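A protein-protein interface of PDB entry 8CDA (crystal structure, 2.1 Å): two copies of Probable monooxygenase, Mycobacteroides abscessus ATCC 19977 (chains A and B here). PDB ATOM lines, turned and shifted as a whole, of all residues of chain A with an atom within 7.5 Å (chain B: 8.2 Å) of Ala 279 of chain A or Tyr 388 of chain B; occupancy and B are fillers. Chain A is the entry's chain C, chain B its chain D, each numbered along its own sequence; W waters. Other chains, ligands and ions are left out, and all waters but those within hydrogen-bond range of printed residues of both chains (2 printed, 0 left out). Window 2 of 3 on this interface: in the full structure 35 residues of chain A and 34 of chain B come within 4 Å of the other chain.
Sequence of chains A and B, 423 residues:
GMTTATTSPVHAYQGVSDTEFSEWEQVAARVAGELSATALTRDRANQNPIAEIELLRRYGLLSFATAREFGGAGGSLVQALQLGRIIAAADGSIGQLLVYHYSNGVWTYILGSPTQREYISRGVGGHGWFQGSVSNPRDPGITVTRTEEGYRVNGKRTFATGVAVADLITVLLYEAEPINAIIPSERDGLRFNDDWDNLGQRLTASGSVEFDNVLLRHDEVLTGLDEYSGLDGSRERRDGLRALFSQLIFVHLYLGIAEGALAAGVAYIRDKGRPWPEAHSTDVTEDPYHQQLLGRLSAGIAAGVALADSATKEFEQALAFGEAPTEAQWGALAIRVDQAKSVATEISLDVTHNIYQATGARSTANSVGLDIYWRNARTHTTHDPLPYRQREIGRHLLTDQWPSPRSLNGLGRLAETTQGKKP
Printed residues of chain A that touch a printed residue of chain B: Trp 276, Glu 278, Ala 279, Asp 287, Pro 288 and Tyr 289. Hydrophobic or aromatic side chains of chain A that line the printed part of chain B: Trp 276, Ala 279, Pro 288 and Tyr 289. Of the 14 printed residues of chain B, 6 touch a printed residue of chain A. Among the printed residues, Asp or Glu carboxylates within 4 Å of a Lys or Arg side-chain nitrogen of the other chain: Glu 278 of chain A with Arg 389 of chain B (3.1 Å).
OH of Tyr 388 of chain B sits at hydrogen-bond distance from OD2 of Asp 287 of chain A (2.5 Å). The side-chain carboxylate (OE1) of Glu 278 of chain A lies within salt-bridge range of the guanidinium group (NH1) of Arg 389 of chain B, 3.1 Å away.
The backbone NH of Tyr 289 of chain A is in hydrogen-bond range of the side-chain carboxylate of Asp 287 of chain A, at 2.8 Å. The guanidinium group of Arg 389 of chain B lies within salt-bridge range of the side-chain carboxylate of Glu 392 of chain B, at 2.8 Å. The guanidinium group of Arg 389 of chain B is in salt-bridge range of the side-chain carboxylate of Asp 338 of chain B. N of His 290 of chain A sits at hydrogen-bond distance from OD1 of Asp 287 of chain A, 2.9 Å away. The side-chain carboxylate of Glu 278 of chain A is in hydrogen-bond range of the indole nitrogen of Trp 276 of chain A (2.6 Å).
Trp 276 of chain A touches Asp 384 of chain B (CH2 to CB, 3.4 Å). CE3 of Trp 276 of chain A touches CD of Pro 385 of chain B, at 3.5 Å. CG of Tyr 388 of chain B touches CD1 of Trp 276 of chain A, at 3.5 Å. CB of Tyr 388 of chain B touches OE1 of Glu 278 of chain A, at 3.6 Å. Ala 279 of chain A touches Tyr 388 of chain B. Tyr 388 of chain B touches Pro 288 of chain A. Tyr 289 of chain A touches Pro 387 of chain B. CE2 of Tyr 388 of chain B touches CD2 of Tyr 289 of chain A, 3.6 Å away. Arg 391 of chain B touches Tyr 289 of chain A.
Pro 275 of chain A touches none of the printed residues of chain B. Of the printed residues of chain B, Glu 278 of chain A touches Tyr 388 (3.6 Å) and Arg 389 (3.1 Å). Ala 279 of chain A touches just one residue of chain B: Tyr 388. Printed residues of chain B within 4 Å of Asp 287 of chain A: Tyr 388. Of the printed residues of chain A, Pro 387 of chain B touches Tyr 289 (3.6 Å). Printed residues of chain A within 4 Å of Tyr 388 of chain B: Trp 276 (3.5 Å), Glu 278 (3.6 Å), Ala 279 (3.3 Å), Asp 287 (2.5 Å), Pro 288 (3.99 Å) and Tyr 289 (3.6 Å). The nearest residue of chain B that does not touch Ala 279 of chain A is Arg 391 of chain B (6.0 Å).
Water W2 lies within hydrogen-bond range of the backbone carbonyl oxygen (O) of Tyr 388 of chain B (2.9 Å), the guanidinium group (NH1) of Arg 391 of chain B (2.9 Å) and the side-chain carboxylate (OE2) of Glu 278 of chain A (3.0 Å). Water W1 bridges N of His 280 of chain A (3.0 Å) and OH of Tyr 388 of chain B (3.0 Å).
No position is printed for both chains.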
ATOM      1  N   PRO A 275      16.033 -17.200   4.490  1.00  0.00           N
ATOM      2  CA  PRO A 275      15.134 -18.327   4.227  1.00  0.00           C
ATOM      3  C   PRO A 275      13.924 -17.885   3.423  1.00  0.00           C
ATOM      4  O   PRO A 275      13.469 -16.742   3.515  1.00  0.00           O
ATOM      5  CB  PRO A 275      14.721 -18.780   5.631  1.00  0.00           C
ATOM      6  CG  PRO A 275      14.830 -17.537   6.459  1.00  0.00           C
ATOM      7  CD  PRO A 275      16.012 -16.788   5.904  1.00  0.00           C
ATOM      8  N   TRP A 276      13.413 -18.805   2.621  1.00  0.00           N
ATOM      9  CA  TRP A 276      12.178 -18.553   1.893  1.00  0.00           C
ATOM     10  C   TRP A 276      10.986 -18.757   2.829  1.00  0.00           C
ATOM     11  O   TRP A 276      10.967 -19.715   3.604  1.00  0.00           O
ATOM     12  CB  TRP A 276      12.078 -19.503   0.698  1.00  0.00           C
ATOM     13  CG  TRP A 276      10.852 -19.326  -0.144  1.00  0.00           C
ATOM     14  CD1 TRP A 276       9.868 -20.246  -0.359  1.00  0.00           C
ATOM     15  CD2 TRP A 276      10.478 -18.159  -0.891  1.00  0.00           C
ATOM     16  NE1 TRP A 276       8.904 -19.726  -1.186  1.00  0.00           N
ATOM     17  CE2 TRP A 276       9.254 -18.447  -1.528  1.00  0.00           C
ATOM     18  CE3 TRP A 276      11.058 -16.902  -1.080  1.00  0.00           C
ATOM     19  CZ2 TRP A 276       8.600 -17.522  -2.338  1.00  0.00           C
ATOM     20  CZ3 TRP A 276      10.405 -15.984  -1.884  1.00  0.00           C
ATOM     21  CH2 TRP A 276       9.189 -16.300  -2.502  1.00  0.00           C
ATOM     22  N   PRO A 277      10.000 -17.855   2.802  1.00  0.00           N
ATOM     23  CA  PRO A 277       8.867 -17.979   3.738  1.00  0.00           C
ATOM     24  C   PRO A 277       8.109 -19.295   3.648  1.00  0.00           C
ATOM     25  O   PRO A 277       7.581 -19.757   4.668  1.00  0.00           O
ATOM     26  CB  PRO A 277       7.983 -16.778   3.376  1.00  0.00           C
ATOM     27  CG  PRO A 277       8.944 -15.768   2.847  1.00  0.00           C
ATOM     28  CD  PRO A 277       9.998 -16.555   2.109  1.00  0.00           C
ATOM     29  N   GLU A 278       8.029 -19.914   2.471  1.00  0.00           N
ATOM     30  CA  GLU A 278       7.363 -21.206   2.354  1.00  0.00           C
ATOM     31  C   GLU A 278       8.201 -22.357   2.895  1.00  0.00           C
ATOM     32  O   GLU A 278       7.663 -23.453   3.083  1.00  0.00           O
ATOM     33  CB  GLU A 278       6.988 -21.499   0.896  1.00  0.00           C
ATOM     34  CG  GLU A 278       5.876 -20.631   0.326  1.00  0.00           C
ATOM     35  CD  GLU A 278       5.667 -20.868  -1.161  1.00  0.00           C
ATOM     36  OE1 GLU A 278       6.598 -20.587  -1.945  1.00  0.00           O
ATOM     37  OE2 GLU A 278       4.580 -21.348  -1.549  1.00  0.00           O
ATOM     38  N   ALA A 279       9.489 -22.142   3.145  1.00  0.00           N
ATOM     39  CA  ALA A 279      10.347 -23.220   3.611  1.00  0.00           C
ATOM     40  C   ALA A 279       9.931 -23.684   5.005  1.00  0.00           C
ATOM     41  O   ALA A 279       9.309 -22.951   5.780  1.00  0.00           O
ATOM     42  CB  ALA A 279      11.810 -22.775   3.627  1.00  0.00           C
ATOM     43  N   HIS A 280      10.286 -24.931   5.316  1.00  0.00           N
ATOM     44  CA  HIS A 280       9.964 -25.487   6.626  1.00  0.00           C
ATOM     45  C   HIS A 280      10.810 -24.853   7.724  1.00  0.00           C
ATOM     46  O   HIS A 280      10.323 -24.626   8.838  1.00  0.00           O
ATOM     47  CB  HIS A 280      10.151 -27.004   6.607  1.00  0.00           C
ATOM     48  CG  HIS A 280      10.473 -27.585   7.949  1.00  0.00           C
ATOM     49  ND1 HIS A 280       9.632 -27.461   9.034  1.00  0.00           N
ATOM     50  CD2 HIS A 280      11.550 -28.281   8.384  1.00  0.00           C
ATOM     51  CE1 HIS A 280      10.175 -28.061  10.080  1.00  0.00           C
ATOM     52  NE2 HIS A 280      11.338 -28.567   9.711  1.00  0.00           N
ATOM     53  N   SER A 281      12.072 -24.558   7.433  1.00  0.00           N
ATOM     54  CA  SER A 281      13.007 -24.041   8.419  1.00  0.00           C
ATOM     55  C   SER A 281      13.244 -22.552   8.200  1.00  0.00           C
ATOM     56  O   SER A 281      13.226 -22.062   7.067  1.00  0.00           O
ATOM     57  CB  SER A 281      14.345 -24.784   8.333  1.00  0.00           C
ATOM     58  OG  SER A 281      15.336 -24.163   9.134  1.00  0.00           O
ATOM     59  N   THR A 282      13.462 -21.836   9.302  1.00  0.00           N
ATOM     60  CA  THR A 282      13.894 -20.446   9.238  1.00  0.00           C
ATOM     61  C   THR A 282      15.394 -20.309   9.010  1.00  0.00           C
ATOM     62  O   THR A 282      15.896 -19.183   8.939  1.00  0.00           O
ATOM     63  CB  THR A 282      13.489 -19.702  10.515  1.00  0.00           C
ATOM     64  OG1 THR A 282      14.069 -20.349  11.653  1.00  0.00           O
ATOM     65  CG2 THR A 282      11.977 -19.685  10.664  1.00  0.00           C
ATOM     66  N   ASP A 283      16.114 -21.423   8.897  1.00  0.00           N
ATOM     67  CA  ASP A 283      17.545 -21.425   8.623  1.00  0.00           C
ATOM     68  C   ASP A 283      17.739 -21.668   7.131  1.00  0.00           C
ATOM     69  O   ASP A 283      17.357 -22.724   6.616  1.00  0.00           O
ATOM     70  CB  ASP A 283      18.226 -22.522   9.443  1.00  0.00           C
ATOM     71  CG  ASP A 283      19.743 -22.499   9.327  1.00  0.00           C
ATOM     72  OD1 ASP A 283      20.287 -21.713   8.522  1.00  0.00           O
ATOM     73  OD2 ASP A 283      20.395 -23.279  10.052  1.00  0.00           O
ATOM     74  N   VAL A 284      18.334 -20.689   6.442  1.00  0.00           N
ATOM     75  CA  VAL A 284      18.528 -20.803   4.998  1.00  0.00           C
ATOM     76  C   VAL A 284      19.465 -21.956   4.653  1.00  0.00           C
ATOM     77  O   VAL A 284      19.367 -22.540   3.569  1.00  0.00           O
ATOM     78  CB  VAL A 284      18.990 -19.460   4.397  1.00  0.00           C
ATOM     79  CG1 VAL A 284      20.393 -19.105   4.877  1.00  0.00           C
ATOM     80  CG2 VAL A 284      18.933 -19.497   2.872  1.00  0.00           C
ATOM     81  N   GLU A 286      19.373 -24.844   5.875  1.00  0.00           N
ATOM     82  CA  GLU A 286      18.620 -26.088   5.950  1.00  0.00           C
ATOM     83  C   GLU A 286      17.645 -26.272   4.794  1.00  0.00           C
ATOM     84  O   GLU A 286      16.892 -27.249   4.790  1.00  0.00           O
ATOM     85  CB  GLU A 286      17.864 -26.177   7.281  1.00  0.00           C
ATOM     86  CG  GLU A 286      18.762 -26.145   8.511  1.00  0.00           C
ATOM     87  CD  GLU A 286      19.656 -27.367   8.615  1.00  0.00           C
ATOM     88  OE1 GLU A 286      19.374 -28.377   7.934  1.00  0.00           O
ATOM     89  OE2 GLU A 286      20.643 -27.318   9.378  1.00  0.00           O
ATOM     90  N   ASP A 287      17.638 -25.362   3.827  1.00  0.00           N
ATOM     91  CA  ASP A 287      16.702 -25.463   2.719  1.00  0.00           C
ATOM     92  C   ASP A 287      16.986 -26.736   1.926  1.00  0.00           C
ATOM     93  O   ASP A 287      18.134 -26.961   1.515  1.00  0.00           O
ATOM     94  CB  ASP A 287      16.828 -24.233   1.821  1.00  0.00           C
ATOM     95  CG  ASP A 287      15.814 -24.227   0.687  1.00  0.00           C
ATOM     96  OD1 ASP A 287      16.005 -24.976  -0.290  1.00  0.00           O
ATOM     97  OD2 ASP A 287      14.817 -23.478   0.780  1.00  0.00           O
ATOM     98  N   PRO A 288      15.986 -27.596   1.706  1.00  0.00           N
ATOM     99  CA  PRO A 288      16.264 -28.877   1.040  1.00  0.00           C
ATOM    100  C   PRO A 288      16.666 -28.729  -0.413  1.00  0.00           C
ATOM    101  O   PRO A 288      17.373 -29.599  -0.936  1.00  0.00           O
ATOM    102  CB  PRO A 288      14.944 -29.648   1.188  1.00  0.00           C
ATOM    103  CG  PRO A 288      13.906 -28.578   1.291  1.00  0.00           C
ATOM    104  CD  PRO A 288      14.564 -27.460   2.069  1.00  0.00           C
ATOM    105  N   TYR A 289      16.233 -27.662  -1.083  1.00  0.00           N
ATOM    106  CA  TYR A 289      16.577 -27.483  -2.489  1.00  0.00           C
ATOM    107  C   TYR A 289      17.952 -26.852  -2.667  1.00  0.00           C
ATOM    108  O   TYR A 289      18.657 -27.179  -3.628  1.00  0.00           O
ATOM    109  CB  TYR A 289      15.496 -26.667  -3.196  1.00  0.00           C
ATOM    110  CG  TYR A 289      14.120 -27.254  -3.012  1.00  0.00           C
ATOM    111  CD1 TYR A 289      13.826 -28.532  -3.466  1.00  0.00           C
ATOM    112  CD2 TYR A 289      13.113 -26.535  -2.379  1.00  0.00           C
ATOM    113  CE1 TYR A 289      12.564 -29.082  -3.294  1.00  0.00           C
ATOM    114  CE2 TYR A 289      11.847 -27.076  -2.207  1.00  0.00           C
ATOM    115  CZ  TYR A 289      11.582 -28.347  -2.664  1.00  0.00           C
ATOM    116  OH  TYR A 289      10.325 -28.887  -2.497  1.00  0.00           O
ATOM    117  N   HIS A 290      18.348 -25.958  -1.758  1.00  0.00           N
ATOM    118  CA  HIS A 290      19.719 -25.463  -1.769  1.00  0.00           C
ATOM    119  C   HIS A 290      20.699 -26.614  -1.596  1.00  0.00           C
ATOM    120  O   HIS A 290      21.649 -26.759  -2.372  1.00  0.00           O
ATOM    121  CB  HIS A 290      19.914 -24.431  -0.655  1.00  0.00           C
ATOM    122  CG  HIS A 290      19.153 -23.160  -0.863  1.00  0.00           C
ATOM    123  ND1 HIS A 290      18.450 -22.893  -2.018  1.00  0.00           N
ATOM    124  CD2 HIS A 290      18.985 -22.081  -0.062  1.00  0.00           C
ATOM    125  CE1 HIS A 290      17.884 -21.703  -1.921  1.00  0.00           C
ATOM    126  NE2 HIS A 290      18.194 -21.189  -0.743  1.00  0.00           N
ATOM    127  N   ASP B 338       1.467 -21.638 -11.759  1.00  0.00           N
ATOM    128  CA  ASP B 338       2.712 -22.286 -11.352  1.00  0.00           C
ATOM    129  C   ASP B 338       3.309 -23.099 -12.491  1.00  0.00           C
ATOM    130  O   ASP B 338       4.524 -23.065 -12.718  1.00  0.00           O
ATOM    131  CB  ASP B 338       2.469 -23.200 -10.154  1.00  0.00           C
ATOM    132  CG  ASP B 338       2.223 -22.440  -8.874  1.00  0.00           C
ATOM    133  OD1 ASP B 338       2.616 -21.258  -8.789  1.00  0.00           O
ATOM    134  OD2 ASP B 338       1.642 -23.040  -7.946  1.00  0.00           O
ATOM    135  N   ASP B 384      11.283 -15.217  -7.089  1.00  0.00           N
ATOM    136  CA  ASP B 384      10.911 -16.206  -6.098  1.00  0.00           C
ATOM    137  C   ASP B 384      11.451 -17.552  -6.561  1.00  0.00           C
ATOM    138  O   ASP B 384      11.543 -17.793  -7.770  1.00  0.00           O
ATOM    139  CB  ASP B 384       9.388 -16.266  -5.898  1.00  0.00           C
ATOM    140  CG  ASP B 384       8.626 -16.413  -7.197  1.00  0.00           C
ATOM    141  OD1 ASP B 384       8.528 -15.423  -7.952  1.00  0.00           O
ATOM    142  OD2 ASP B 384       8.125 -17.525  -7.462  1.00  0.00           O
ATOM    143  N   PRO B 385      11.845 -18.429  -5.638  1.00  0.00           N
ATOM    144  CA  PRO B 385      12.575 -19.642  -6.039  1.00  0.00           C
ATOM    145  C   PRO B 385      11.706 -20.606  -6.834  1.00  0.00           C
ATOM    146  O   PRO B 385      10.617 -20.992  -6.399  1.00  0.00           O
ATOM    147  CB  PRO B 385      13.025 -20.252  -4.705  1.00  0.00           C
ATOM    148  CG  PRO B 385      12.115 -19.653  -3.680  1.00  0.00           C
ATOM    149  CD  PRO B 385      11.790 -18.275  -4.175  1.00  0.00           C
ATOM    150  N   LEU B 386      12.213 -20.996  -8.003  1.00  0.00           N
ATOM    151  CA  LEU B 386      11.539 -21.971  -8.862  1.00  0.00           C
ATOM    152  C   LEU B 386      11.125 -23.256  -8.151  1.00  0.00           C
ATOM    153  O   LEU B 386       9.969 -23.676  -8.325  1.00  0.00           O
ATOM    154  CB  LEU B 386      12.397 -22.260 -10.103  1.00  0.00           C
ATOM    155  CG  LEU B 386      11.867 -23.365 -11.020  1.00  0.00           C
ATOM    156  CD1 LEU B 386      10.517 -22.963 -11.598  1.00  0.00           C
ATOM    157  CD2 LEU B 386      12.858 -23.692 -12.131  1.00  0.00           C
ATOM    158  N   PRO B 387      11.985 -23.927  -7.370  1.00  0.00           N
ATOM    159  CA  PRO B 387      11.564 -25.205  -6.766  1.00  0.00           C
ATOM    160  C   PRO B 387      10.321 -25.114  -5.894  1.00  0.00           C
ATOM    161  O   PRO B 387       9.591 -26.105  -5.776  1.00  0.00           O
ATOM    162  CB  PRO B 387      12.798 -25.654  -5.966  1.00  0.00           C
ATOM    163  CG  PRO B 387      13.641 -24.430  -5.824  1.00  0.00           C
ATOM    164  CD  PRO B 387      13.398 -23.633  -7.064  1.00  0.00           C
ATOM    165  N   TYR B 388      10.047 -23.958  -5.286  1.00  0.00           N
ATOM    166  CA  TYR B 388       8.857 -23.847  -4.450  1.00  0.00           C
ATOM    167  C   TYR B 388       7.585 -23.666  -5.269  1.00  0.00           C
ATOM    168  O   TYR B 388       6.502 -24.052  -4.814  1.00  0.00           O
ATOM    169  CB  TYR B 388       9.032 -22.746  -3.407  1.00  0.00           C
ATOM    170  CG  TYR B 388       9.950 -23.155  -2.278  1.00  0.00           C
ATOM    171  CD1 TYR B 388       9.455 -23.844  -1.176  1.00  0.00           C
ATOM    172  CD2 TYR B 388      11.310 -22.868  -2.316  1.00  0.00           C
ATOM    173  CE1 TYR B 388      10.285 -24.226  -0.142  1.00  0.00           C
ATOM    174  CE2 TYR B 388      12.151 -23.246  -1.282  1.00  0.00           C
ATOM    175  CZ  TYR B 388      11.631 -23.925  -0.197  1.00  0.00           C
ATOM    176  OH  TYR B 388      12.450 -24.313   0.834  1.00  0.00           O
ATOM    177  N   ARG B 389       7.687 -23.096  -6.473  1.00  0.00           N
ATOM    178  CA  ARG B 389       6.533 -23.072  -7.365  1.00  0.00           C
ATOM    179  C   ARG B 389       6.245 -24.462  -7.915  1.00  0.00           C
ATOM    180  O   ARG B 389       5.080 -24.851  -8.060  1.00  0.00           O
ATOM    181  CB  ARG B 389       6.754 -22.069  -8.499  1.00  0.00           C
ATOM    182  CG  ARG B 389       7.001 -20.640  -8.036  1.00  0.00           C
ATOM    183  CD  ARG B 389       5.709 -19.853  -7.799  1.00  0.00           C
ATOM    184  NE  ARG B 389       4.804 -20.505  -6.857  1.00  0.00           N
ATOM    185  CZ  ARG B 389       4.965 -20.513  -5.540  1.00  0.00           C
ATOM    186  NH1 ARG B 389       6.001 -19.923  -4.964  1.00  0.00           N
ATOM    187  NH2 ARG B 389       4.066 -21.133  -4.781  1.00  0.00           N
ATOM    188  N   GLN B 390       7.296 -25.224  -8.222  1.00  0.00           N
ATOM    189  CA  GLN B 390       7.112 -26.609  -8.636  1.00  0.00           C
ATOM    190  C   GLN B 390       6.604 -27.463  -7.480  1.00  0.00           C
ATOM    191  O   GLN B 390       5.754 -28.339  -7.674  1.00  0.00           O
ATOM    192  CB  GLN B 390       8.428 -27.163  -9.192  1.00  0.00           C
ATOM    193  CG  GLN B 390       8.959 -26.405 -10.407  1.00  0.00           C
ATOM    194  CD  GLN B 390      10.352 -26.851 -10.823  1.00  0.00           C
ATOM    195  OE1 GLN B 390      11.139 -27.318  -9.999  1.00  0.00           O
ATOM    196  NE2 GLN B 390      10.661 -26.710 -12.107  1.00  0.00           N
ATOM    197  N   ARG B 391       7.107 -27.209  -6.268  1.00  0.00           N
ATOM    198  CA  ARG B 391       6.658 -27.954  -5.096  1.00  0.00           C
ATOM    199  C   ARG B 391       5.159 -27.790  -4.870  1.00  0.00           C
ATOM    200  O   ARG B 391       4.483 -28.729  -4.435  1.00  0.00           O
ATOM    201  CB  ARG B 391       7.427 -27.485  -3.859  1.00  0.00           C
ATOM    202  CG  ARG B 391       6.852 -27.977  -2.543  1.00  0.00           C
ATOM    203  CD  ARG B 391       7.593 -27.389  -1.354  1.00  0.00           C
ATOM    204  NE  ARG B 391       7.005 -27.814  -0.088  1.00  0.00           N
ATOM    205  CZ  ARG B 391       6.158 -27.086   0.627  1.00  0.00           C
ATOM    206  NH1 ARG B 391       5.806 -25.867   0.252  1.00  0.00           N
ATOM    207  NH2 ARG B 391       5.652 -27.594   1.747  1.00  0.00           N
ATOM    208  N   GLU B 392       4.623 -26.600  -5.151  1.00  0.00           N
ATOM    209  CA  GLU B 392       3.203 -26.360  -4.911  1.00  0.00           C
ATOM    210  C   GLU B 392       2.341 -27.231  -5.817  1.00  0.00           C
ATOM    211  O   GLU B 392       1.309 -27.758  -5.384  1.00  0.00           O
ATOM    212  CB  GLU B 392       2.880 -24.876  -5.091  1.00  0.00           C
ATOM    213  CG  GLU B 392       1.545 -24.456  -4.500  1.00  0.00           C
ATOM    214  CD  GLU B 392       1.402 -22.948  -4.385  1.00  0.00           C
ATOM    215  OE1 GLU B 392       1.617 -22.247  -5.394  1.00  0.00           O
ATOM    216  OE2 GLU B 392       1.083 -22.461  -3.279  1.00  0.00           O
ATOM    217  N   ILE B 393       2.761 -27.411  -7.072  1.00  0.00           N
ATOM    218  CA  ILE B 393       2.051 -28.304  -7.986  1.00  0.00           C
ATOM    219  C   ILE B 393       2.076 -29.734  -7.459  1.00  0.00           C
ATOM    220  O   ILE B 393       1.033 -30.387  -7.329  1.00  0.00           O
ATOM    221  CB  ILE B 393       2.652 -28.208  -9.402  1.00  0.00           C
ATOM    222  CG1 ILE B 393       2.658 -26.758  -9.889  1.00  0.00           C
ATOM    223  CG2 ILE B 393       1.891 -29.105 -10.376  1.00  0.00           C
ATOM    224  CD1 ILE B 393       3.545 -26.531 -11.101  1.00  0.00           C
ATOM    225  N   GLY B 394       3.272 -30.241  -7.145  1.00  0.00           N
ATOM    226  CA  GLY B 394       3.385 -31.611  -6.672  1.00  0.00           C
ATOM    227  C   GLY B 394       2.695 -31.842  -5.343  1.00  0.00           C
ATOM    228  O   GLY B 394       2.145 -32.920  -5.106  1.00  0.00           O
ATOM    229  N   ARG B 395       2.712 -30.837  -4.463  1.00  0.00           N
ATOM    230  CA  ARG B 395       2.026 -30.959  -3.180  1.00  0.00           C
ATOM    231  C   ARG B 395       0.520 -31.121  -3.369  1.00  0.00           C
ATOM    232  O   ARG B 395      -0.126 -31.877  -2.635  1.00  0.00           O
ATOM    233  CB  ARG B 395       2.332 -29.741  -2.312  1.00  0.00           C
ATOM    234  CG  ARG B 395       1.574 -29.706  -1.006  1.00  0.00           C
ATOM    235  CD  ARG B 395       1.911 -28.458  -0.207  1.00  0.00           C
ATOM    236  NE  ARG B 395       1.091 -28.366   0.993  1.00  0.00           N
ATOM    237  CZ  ARG B 395       1.327 -29.043   2.107  1.00  0.00           C
ATOM    238  NH1 ARG B 395       2.355 -29.870   2.205  1.00  0.00           N
ATOM    239  NH2 ARG B 395       0.510 -28.891   3.146  1.00  0.00           N
ATOM    240  N   ARG B 406      -1.680 -16.775   0.303  1.00  0.00           N
ATOM    241  CA  ARG B 406      -0.747 -16.831   1.423  1.00  0.00           C
ATOM    242  C   ARG B 406      -0.386 -15.430   1.908  1.00  0.00           C
ATOM    243  O   ARG B 406      -0.841 -14.991   2.965  1.00  0.00           O
ATOM    244  CB  ARG B 406       0.523 -17.590   1.028  1.00  0.00           C
ATOM    245  CG  ARG B 406       1.542 -16.753   0.269  1.00  0.00           C
ATOM    246  CD  ARG B 406       2.719 -17.599  -0.201  1.00  0.00           C
ATOM    247  NE  ARG B 406       4.003 -16.996   0.141  1.00  0.00           N
ATOM    248  CZ  ARG B 406       4.615 -16.069  -0.584  1.00  0.00           C
ATOM    249  NH1 ARG B 406       4.084 -15.605  -1.704  1.00  0.00           N
ATOM    250  NH2 ARG B 406       5.789 -15.596  -0.176  1.00  0.00           N
HETATM  251  O   HOH W   1      11.475 -26.243   2.933  1.00  0.00           O
HETATM  252  O   HOH W   2       5.698 -24.052  -2.050  1.00  0.00           O
